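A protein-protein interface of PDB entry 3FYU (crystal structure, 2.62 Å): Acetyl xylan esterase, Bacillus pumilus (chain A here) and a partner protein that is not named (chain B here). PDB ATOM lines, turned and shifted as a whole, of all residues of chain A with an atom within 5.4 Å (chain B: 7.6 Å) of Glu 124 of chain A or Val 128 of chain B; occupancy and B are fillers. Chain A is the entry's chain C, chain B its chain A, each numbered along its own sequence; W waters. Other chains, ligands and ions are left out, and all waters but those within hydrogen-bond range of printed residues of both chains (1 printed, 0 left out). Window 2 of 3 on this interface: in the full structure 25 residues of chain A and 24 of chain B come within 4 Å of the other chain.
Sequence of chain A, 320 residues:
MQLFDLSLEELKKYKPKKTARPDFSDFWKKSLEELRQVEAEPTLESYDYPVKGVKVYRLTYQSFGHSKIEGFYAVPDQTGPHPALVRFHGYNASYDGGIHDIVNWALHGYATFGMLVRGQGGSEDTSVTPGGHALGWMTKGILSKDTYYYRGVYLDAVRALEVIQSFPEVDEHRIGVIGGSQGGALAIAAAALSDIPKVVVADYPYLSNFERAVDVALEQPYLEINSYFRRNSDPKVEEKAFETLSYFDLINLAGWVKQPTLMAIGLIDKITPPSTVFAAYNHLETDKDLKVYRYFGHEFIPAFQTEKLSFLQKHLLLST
Glu 124 of chain A touches just these residues of chain B: Val 128 (3.7 Å), Thr 129 (3.3 Å) and Pro 130 (3.5 Å).
Of chain A, only Glu 124, Asp 125 and Thr 126 come within 4 Å of Val 128 of chain B.
Of the printed residues of chain B, Gly 119 of chain A touches Thr 129, Gly 131 and Gly 132.
Printed residues of chain B within 4 Å of Ser 123 of chain A: Gly 131 and Gly 132.
Thr 147 of chain B touches none of the printed residues of chain A.
Tyr 148 of chain B touches none of the printed residues of chain A.
The nearest printed residue of chain A that does not touch Val 128 of chain B is Ser 67 of chain A (6.4 Å).
Among the printed residues, merely in contact across the chains: Gly 119 of chain A with Thr 129 of chain B, Gly 119 of chain A with Gly 131 of chain B, Gly 119 of chain A with Gly 132 of chain B, Gly 122 of chain A with Gly 132 of chain B, Ser 123 of chain A with Gly 131 of chain B, Ser 123 of chain A with Gly 132 of chain B, Glu 124 of chain A with Val 128 of chain B, Glu 124 of chain A with Thr 129 of chain B, Glu 124 of chain A with Pro 130 of chain B, Asp 125 of chain A with Val 128 of chain B and Thr 126 of chain A with Val 128 of chain B.
Of the 14 printed residues of chain B, 5 touch a printed residue of chain A.
Printed residues of chain B that touch a printed residue of chain A: Val 128, Thr 129, Pro 130, Gly 131 and Gly 132.
Of the 12 printed residues of chain A, 6 touch a printed residue of chain B.
Among the printed residues, 12 pairs touch across the chains.
Among the printed residues, no Asp or Glu carboxylate lies within 4 Å of a Lys or Arg side-chain nitrogen of the other chain.
OG1 of Thr 126 of chain A lies within hydrogen-bond range of OG of Ser 67 of chain A (2.8 Å).
The backbone NH (N) of Lys 68 of chain A is in hydrogen-bond range of the side-chain carboxylate (OE1) of Glu 124 of chain A (2.7 Å).
The guanidinium group (NH1) of Arg 118 of chain A is in salt-bridge range of the side-chain carboxylate (OD1) of Asp 125 of chain A (3.1 Å).
O of Thr 129 of chain B sits at hydrogen-bond distance from N of Asp 125 of chain A (2.9 Å).
Water W1 lies within hydrogen-bond range of the side-chain hydroxyl of Thr 129 of chain B (2.7 Å) and the backbone carbonyl oxygen of Asp 125 of chain A (3.1 Å).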
ATOM      1  N   GLN A  62     -30.069 -21.180 -28.909  1.00  0.00           N
ATOM      2  CA  GLN A  62     -28.727 -21.440 -29.400  1.00  0.00           C
ATOM      3  C   GLN A  62     -28.771 -21.519 -30.920  1.00  0.00           C
ATOM      4  O   GLN A  62     -29.705 -22.082 -31.497  1.00  0.00           O
ATOM      5  CB  GLN A  62     -28.218 -22.745 -28.806  1.00  0.00           C
ATOM      6  CG  GLN A  62     -28.207 -22.739 -27.299  1.00  0.00           C
ATOM      7  CD  GLN A  62     -27.340 -21.620 -26.749  1.00  0.00           C
ATOM      8  OE1 GLN A  62     -26.143 -21.544 -27.043  1.00  0.00           O
ATOM      9  NE2 GLN A  62     -27.945 -20.737 -25.952  1.00  0.00           N
ATOM     10  N   HIS A  66     -22.930 -22.036 -31.735  1.00  0.00           N
ATOM     11  CA  HIS A  66     -23.349 -22.138 -30.343  1.00  0.00           C
ATOM     12  C   HIS A  66     -23.524 -20.758 -29.705  1.00  0.00           C
ATOM     13  O   HIS A  66     -23.302 -20.575 -28.506  1.00  0.00           O
ATOM     14  CB  HIS A  66     -22.328 -22.961 -29.555  1.00  0.00           C
ATOM     15  CG  HIS A  66     -22.278 -24.399 -29.965  1.00  0.00           C
ATOM     16  ND1 HIS A  66     -23.264 -25.304 -29.629  1.00  0.00           N
ATOM     17  CD2 HIS A  66     -21.386 -25.078 -30.723  1.00  0.00           C
ATOM     18  CE1 HIS A  66     -22.980 -26.479 -30.162  1.00  0.00           C
ATOM     19  NE2 HIS A  66     -21.846 -26.367 -30.831  1.00  0.00           N
ATOM     20  N   SER A  67     -23.919 -19.789 -30.518  1.00  0.00           N
ATOM     21  CA  SER A  67     -24.141 -18.440 -30.032  1.00  0.00           C
ATOM     22  C   SER A  67     -25.533 -18.346 -29.421  1.00  0.00           C
ATOM     23  O   SER A  67     -26.483 -18.916 -29.942  1.00  0.00           O
ATOM     24  CB  SER A  67     -24.024 -17.438 -31.181  1.00  0.00           C
ATOM     25  OG  SER A  67     -22.712 -17.419 -31.713  1.00  0.00           O
ATOM     26  N   LYS A  68     -25.650 -17.634 -28.305  1.00  0.00           N
ATOM     27  CA  LYS A  68     -26.936 -17.459 -27.651  1.00  0.00           C
ATOM     28  C   LYS A  68     -27.592 -16.197 -28.200  1.00  0.00           C
ATOM     29  O   LYS A  68     -27.137 -15.084 -27.937  1.00  0.00           O
ATOM     30  CB  LYS A  68     -26.744 -17.337 -26.147  1.00  0.00           C
ATOM     31  CG  LYS A  68     -28.036 -17.333 -25.368  1.00  0.00           C
ATOM     32  CD  LYS A  68     -27.752 -17.440 -23.885  1.00  0.00           C
ATOM     33  CE  LYS A  68     -29.036 -17.563 -23.079  1.00  0.00           C
ATOM     34  NZ  LYS A  68     -28.779 -17.671 -21.612  1.00  0.00           N
ATOM     35  N   ILE A  69     -28.655 -16.387 -28.979  1.00  0.00           N
ATOM     36  CA  ILE A  69     -29.401 -15.284 -29.583  1.00  0.00           C
ATOM     37  C   ILE A  69     -30.581 -14.890 -28.700  1.00  0.00           C
ATOM     38  O   ILE A  69     -31.237 -15.753 -28.122  1.00  0.00           O
ATOM     39  CB  ILE A  69     -29.918 -15.687 -30.971  1.00  0.00           C
ATOM     40  CG1 ILE A  69     -28.758 -16.257 -31.792  1.00  0.00           C
ATOM     41  CG2 ILE A  69     -30.527 -14.499 -31.673  1.00  0.00           C
ATOM     42  CD1 ILE A  69     -27.549 -15.355 -31.859  1.00  0.00           C
ATOM     43  N   ARG A 118     -26.600 -10.310 -33.700  1.00  0.00           N
ATOM     44  CA  ARG A 118     -25.307 -10.531 -33.043  1.00  0.00           C
ATOM     45  C   ARG A 118     -24.446  -9.303 -32.781  1.00  0.00           C
ATOM     46  O   ARG A 118     -24.074  -8.585 -33.710  1.00  0.00           O
ATOM     47  CB  ARG A 118     -24.458 -11.484 -33.869  1.00  0.00           C
ATOM     48  CG  ARG A 118     -25.047 -12.831 -34.075  1.00  0.00           C
ATOM     49  CD  ARG A 118     -24.042 -13.731 -34.743  1.00  0.00           C
ATOM     50  NE  ARG A 118     -24.561 -15.089 -34.866  1.00  0.00           N
ATOM     51  CZ  ARG A 118     -23.811 -16.187 -34.829  1.00  0.00           C
ATOM     52  NH1 ARG A 118     -22.494 -16.092 -34.670  1.00  0.00           N
ATOM     53  NH2 ARG A 118     -24.386 -17.377 -34.942  1.00  0.00           N
ATOM     54  N   GLY A 119     -24.107  -9.090 -31.515  1.00  0.00           N
ATOM     55  CA  GLY A 119     -23.257  -7.970 -31.154  1.00  0.00           C
ATOM     56  C   GLY A 119     -23.810  -6.582 -31.389  1.00  0.00           C
ATOM     57  O   GLY A 119     -23.164  -5.607 -31.017  1.00  0.00           O
ATOM     58  N   GLY A 122     -28.130  -6.766 -29.490  1.00  0.00           N
ATOM     59  CA  GLY A 122     -28.060  -7.794 -28.469  1.00  0.00           C
ATOM     60  C   GLY A 122     -27.548  -9.095 -29.047  1.00  0.00           C
ATOM     61  O   GLY A 122     -27.007  -9.109 -30.152  1.00  0.00           O
ATOM     62  N   SER A 123     -27.720 -10.182 -28.298  1.00  0.00           N
ATOM     63  CA  SER A 123     -27.285 -11.511 -28.712  1.00  0.00           C
ATOM     64  C   SER A 123     -25.775 -11.661 -28.711  1.00  0.00           C
ATOM     65  O   SER A 123     -25.031 -10.699 -28.879  1.00  0.00           O
ATOM     66  CB  SER A 123     -27.834 -11.851 -30.095  1.00  0.00           C
ATOM     67  OG  SER A 123     -29.248 -11.883 -30.070  1.00  0.00           O
ATOM     68  N   GLU A 124     -25.335 -12.894 -28.522  1.00  0.00           N
ATOM     69  CA  GLU A 124     -23.925 -13.226 -28.480  1.00  0.00           C
ATOM     70  C   GLU A 124     -23.395 -13.637 -29.846  1.00  0.00           C
ATOM     71  O   GLU A 124     -24.085 -14.294 -30.622  1.00  0.00           O
ATOM     72  CB  GLU A 124     -23.719 -14.369 -27.483  1.00  0.00           C
ATOM     73  CG  GLU A 124     -22.442 -15.171 -27.670  1.00  0.00           C
ATOM     74  CD  GLU A 124     -22.405 -16.413 -26.790  1.00  0.00           C
ATOM     75  OE1 GLU A 124     -23.371 -17.207 -26.849  1.00  0.00           O
ATOM     76  OE2 GLU A 124     -21.410 -16.606 -26.043  1.00  0.00           O
ATOM     77  N   ASP A 125     -22.165 -13.233 -30.145  1.00  0.00           N
ATOM     78  CA  ASP A 125     -21.536 -13.610 -31.400  1.00  0.00           C
ATOM     79  C   ASP A 125     -20.248 -14.350 -31.041  1.00  0.00           C
ATOM     80  O   ASP A 125     -19.253 -13.729 -30.662  1.00  0.00           O
ATOM     81  CB  ASP A 125     -21.213 -12.389 -32.253  1.00  0.00           C
ATOM     82  CG  ASP A 125     -20.670 -12.775 -33.617  1.00  0.00           C
ATOM     83  OD1 ASP A 125     -20.388 -13.977 -33.812  1.00  0.00           O
ATOM     84  OD2 ASP A 125     -20.521 -11.895 -34.494  1.00  0.00           O
ATOM     85  N   THR A 126     -20.271 -15.676 -31.140  1.00  0.00           N
ATOM     86  CA  THR A 126     -19.086 -16.468 -30.799  1.00  0.00           C
ATOM     87  C   THR A 126     -18.077 -16.500 -31.933  1.00  0.00           C
ATOM     88  O   THR A 126     -16.935 -16.887 -31.730  1.00  0.00           O
ATOM     89  CB  THR A 126     -19.439 -17.919 -30.464  1.00  0.00           C
ATOM     90  OG1 THR A 126     -20.119 -18.494 -31.580  1.00  0.00           O
ATOM     91  CG2 THR A 126     -20.318 -17.993 -29.240  1.00  0.00           C
ATOM     92  N   ARG B 118      -6.036  -6.087 -32.574  1.00  0.00           N
ATOM     93  CA  ARG B 118      -7.113  -7.043 -32.847  1.00  0.00           C
ATOM     94  C   ARG B 118      -8.293  -6.539 -33.664  1.00  0.00           C
ATOM     95  O   ARG B 118      -8.966  -5.575 -33.288  1.00  0.00           O
ATOM     96  CB  ARG B 118      -7.673  -7.588 -31.538  1.00  0.00           C
ATOM     97  CG  ARG B 118      -6.684  -8.321 -30.683  1.00  0.00           C
ATOM     98  CD  ARG B 118      -7.413  -8.977 -29.533  1.00  0.00           C
ATOM     99  NE  ARG B 118      -6.497  -9.726 -28.697  1.00  0.00           N
ATOM    100  CZ  ARG B 118      -6.830 -10.803 -28.006  1.00  0.00           C
ATOM    101  NH1 ARG B 118      -8.072 -11.264 -28.049  1.00  0.00           N
ATOM    102  NH2 ARG B 118      -5.908 -11.424 -27.280  1.00  0.00           N
ATOM    103  N   ASP B 125      -8.853 -11.766 -33.275  1.00  0.00           N
ATOM    104  CA  ASP B 125      -9.438 -11.548 -31.964  1.00  0.00           C
ATOM    105  C   ASP B 125     -10.377 -12.713 -31.728  1.00  0.00           C
ATOM    106  O   ASP B 125     -11.470 -12.765 -32.304  1.00  0.00           O
ATOM    107  CB  ASP B 125     -10.225 -10.237 -31.910  1.00  0.00           C
ATOM    108  CG  ASP B 125     -10.744  -9.935 -30.517  1.00  0.00           C
ATOM    109  OD1 ASP B 125     -10.557 -10.791 -29.630  1.00  0.00           O
ATOM    110  OD2 ASP B 125     -11.339  -8.855 -30.302  1.00  0.00           O
ATOM    111  N   THR B 126      -9.940 -13.657 -30.898  1.00  0.00           N
ATOM    112  CA  THR B 126     -10.750 -14.827 -30.603  1.00  0.00           C
ATOM    113  C   THR B 126     -11.788 -14.559 -29.531  1.00  0.00           C
ATOM    114  O   THR B 126     -12.696 -15.363 -29.328  1.00  0.00           O
ATOM    115  CB  THR B 126      -9.893 -16.007 -30.133  1.00  0.00           C
ATOM    116  OG1 THR B 126      -9.188 -15.652 -28.934  1.00  0.00           O
ATOM    117  CG2 THR B 126      -8.911 -16.399 -31.217  1.00  0.00           C
ATOM    118  N   SER B 127     -11.667 -13.434 -28.838  1.00  0.00           N
ATOM    119  CA  SER B 127     -12.623 -13.129 -27.795  1.00  0.00           C
ATOM    120  C   SER B 127     -14.017 -12.977 -28.385  1.00  0.00           C
ATOM    121  O   SER B 127     -14.237 -12.274 -29.381  1.00  0.00           O
ATOM    122  CB  SER B 127     -12.217 -11.861 -27.044  1.00  0.00           C
ATOM    123  OG  SER B 127     -12.307 -10.719 -27.872  1.00  0.00           O
ATOM    124  N   VAL B 128     -14.951 -13.668 -27.754  1.00  0.00           N
ATOM    125  CA  VAL B 128     -16.349 -13.673 -28.132  1.00  0.00           C
ATOM    126  C   VAL B 128     -17.017 -12.332 -27.811  1.00  0.00           C
ATOM    127  O   VAL B 128     -16.548 -11.587 -26.945  1.00  0.00           O
ATOM    128  CB  VAL B 128     -17.084 -14.807 -27.361  1.00  0.00           C
ATOM    129  CG1 VAL B 128     -18.581 -14.721 -27.573  1.00  0.00           C
ATOM    130  CG2 VAL B 128     -16.569 -16.160 -27.824  1.00  0.00           C
ATOM    131  N   THR B 129     -18.100 -12.025 -28.526  1.00  0.00           N
ATOM    132  CA  THR B 129     -18.876 -10.813 -28.287  1.00  0.00           C
ATOM    133  C   THR B 129     -20.006 -11.278 -27.371  1.00  0.00           C
ATOM    134  O   THR B 129     -20.929 -11.957 -27.817  1.00  0.00           O
ATOM    135  CB  THR B 129     -19.479 -10.281 -29.580  1.00  0.00           C
ATOM    136  OG1 THR B 129     -18.424 -10.005 -30.510  1.00  0.00           O
ATOM    137  CG2 THR B 129     -20.281  -9.021 -29.314  1.00  0.00           C
ATOM    138  N   PRO B 130     -19.942 -10.925 -26.074  1.00  0.00           N
ATOM    139  CA  PRO B 130     -20.953 -11.317 -25.089  1.00  0.00           C
ATOM    140  C   PRO B 130     -22.363 -10.894 -25.463  1.00  0.00           C
ATOM    141  O   PRO B 130     -23.309 -11.658 -25.312  1.00  0.00           O
ATOM    142  CB  PRO B 130     -20.469 -10.644 -23.804  1.00  0.00           C
ATOM    143  CG  PRO B 130     -19.022 -10.548 -23.994  1.00  0.00           C
ATOM    144  CD  PRO B 130     -18.909 -10.101 -25.432  1.00  0.00           C
ATOM    145  N   GLY B 131     -22.498  -9.673 -25.951  1.00  0.00           N
ATOM    146  CA  GLY B 131     -23.810  -9.192 -26.314  1.00  0.00           C
ATOM    147  C   GLY B 131     -23.762  -7.927 -27.143  1.00  0.00           C
ATOM    148  O   GLY B 131     -22.733  -7.585 -27.735  1.00  0.00           O
ATOM    149  N   GLY B 132     -24.889  -7.224 -27.183  1.00  0.00           N
ATOM    150  CA  GLY B 132     -24.965  -6.004 -27.961  1.00  0.00           C
ATOM    151  C   GLY B 132     -24.020  -4.910 -27.495  1.00  0.00           C
ATOM    152  O   GLY B 132     -23.680  -4.793 -26.312  1.00  0.00           O
ATOM    153  N   LYS B 140     -17.270  -3.307 -27.039  1.00  0.00           N
ATOM    154  CA  LYS B 140     -17.341  -4.761 -27.168  1.00  0.00           C
ATOM    155  C   LYS B 140     -16.961  -5.426 -25.842  1.00  0.00           C
ATOM    156  O   LYS B 140     -15.873  -5.206 -25.320  1.00  0.00           O
ATOM    157  CB  LYS B 140     -16.398  -5.243 -28.269  1.00  0.00           C
ATOM    158  CG  LYS B 140     -16.504  -6.724 -28.541  1.00  0.00           C
ATOM    159  CD  LYS B 140     -15.436  -7.225 -29.519  1.00  0.00           C
ATOM    160  CE  LYS B 140     -15.471  -8.763 -29.602  1.00  0.00           C
ATOM    161  NZ  LYS B 140     -14.261  -9.358 -30.236  1.00  0.00           N
ATOM    162  N   GLY B 141     -17.878  -6.218 -25.297  1.00  0.00           N
ATOM    163  CA  GLY B 141     -17.633  -6.914 -24.046  1.00  0.00           C
ATOM    164  C   GLY B 141     -17.462  -5.986 -22.861  1.00  0.00           C
ATOM    165  O   GLY B 141     -16.857  -6.361 -21.863  1.00  0.00           O
ATOM    166  N   THR B 147     -14.215  -9.804 -20.338  1.00  0.00           N
ATOM    167  CA  THR B 147     -14.621  -9.851 -21.733  1.00  0.00           C
ATOM    168  C   THR B 147     -14.300  -8.602 -22.531  1.00  0.00           C
ATOM    169  O   THR B 147     -14.373  -8.618 -23.757  1.00  0.00           O
ATOM    170  CB  THR B 147     -16.146 -10.092 -21.832  1.00  0.00           C
ATOM    171  OG1 THR B 147     -16.841  -9.020 -21.187  1.00  0.00           O
ATOM    172  CG2 THR B 147     -16.532 -11.384 -21.141  1.00  0.00           C
ATOM    173  N   TYR B 148     -13.943  -7.519 -21.846  1.00  0.00           N
ATOM    174  CA  TYR B 148     -13.677  -6.262 -22.528  1.00  0.00           C
ATOM    175  C   TYR B 148     -12.597  -6.300 -23.609  1.00  0.00           C
ATOM    176  O   TYR B 148     -11.492  -6.789 -23.387  1.00  0.00           O
ATOM    177  CB  TYR B 148     -13.356  -5.164 -21.511  1.00  0.00           C
ATOM    178  CG  TYR B 148     -13.348  -3.780 -22.135  1.00  0.00           C
ATOM    179  CD1 TYR B 148     -14.455  -3.316 -22.845  1.00  0.00           C
ATOM    180  CD2 TYR B 148     -12.238  -2.951 -22.029  1.00  0.00           C
ATOM    181  CE1 TYR B 148     -14.462  -2.072 -23.434  1.00  0.00           C
ATOM    182  CE2 TYR B 148     -12.230  -1.690 -22.616  1.00  0.00           C
ATOM    183  CZ  TYR B 148     -13.351  -1.259 -23.318  1.00  0.00           C
ATOM    184  OH  TYR B 148     -13.369  -0.014 -23.906  1.00  0.00           O
ATOM    185  N   TYR B 149     -12.935  -5.751 -24.772  1.00  0.00           N
ATOM    186  CA  TYR B 149     -12.058  -5.710 -25.931  1.00  0.00           C
ATOM    187  C   TYR B 149     -10.583  -5.455 -25.652  1.00  0.00           C
ATOM    188  O   TYR B 149      -9.718  -6.196 -26.109  1.00  0.00           O
ATOM    189  CB  TYR B 149     -12.558  -4.654 -26.913  1.00  0.00           C
ATOM    190  CG  TYR B 149     -11.656  -4.437 -28.109  1.00  0.00           C
ATOM    191  CD1 TYR B 149     -11.509  -5.421 -29.082  1.00  0.00           C
ATOM    192  CD2 TYR B 149     -10.966  -3.234 -28.282  1.00  0.00           C
ATOM    193  CE1 TYR B 149     -10.700  -5.213 -30.207  1.00  0.00           C
ATOM    194  CE2 TYR B 149     -10.152  -3.017 -29.400  1.00  0.00           C
ATOM    195  CZ  TYR B 149     -10.030  -4.012 -30.356  1.00  0.00           C
ATOM    196  OH  TYR B 149      -9.255  -3.796 -31.465  1.00  0.00           O
HETATM  197  O   HOH W   1     -16.999 -11.864 -31.816  1.00  0.00           O
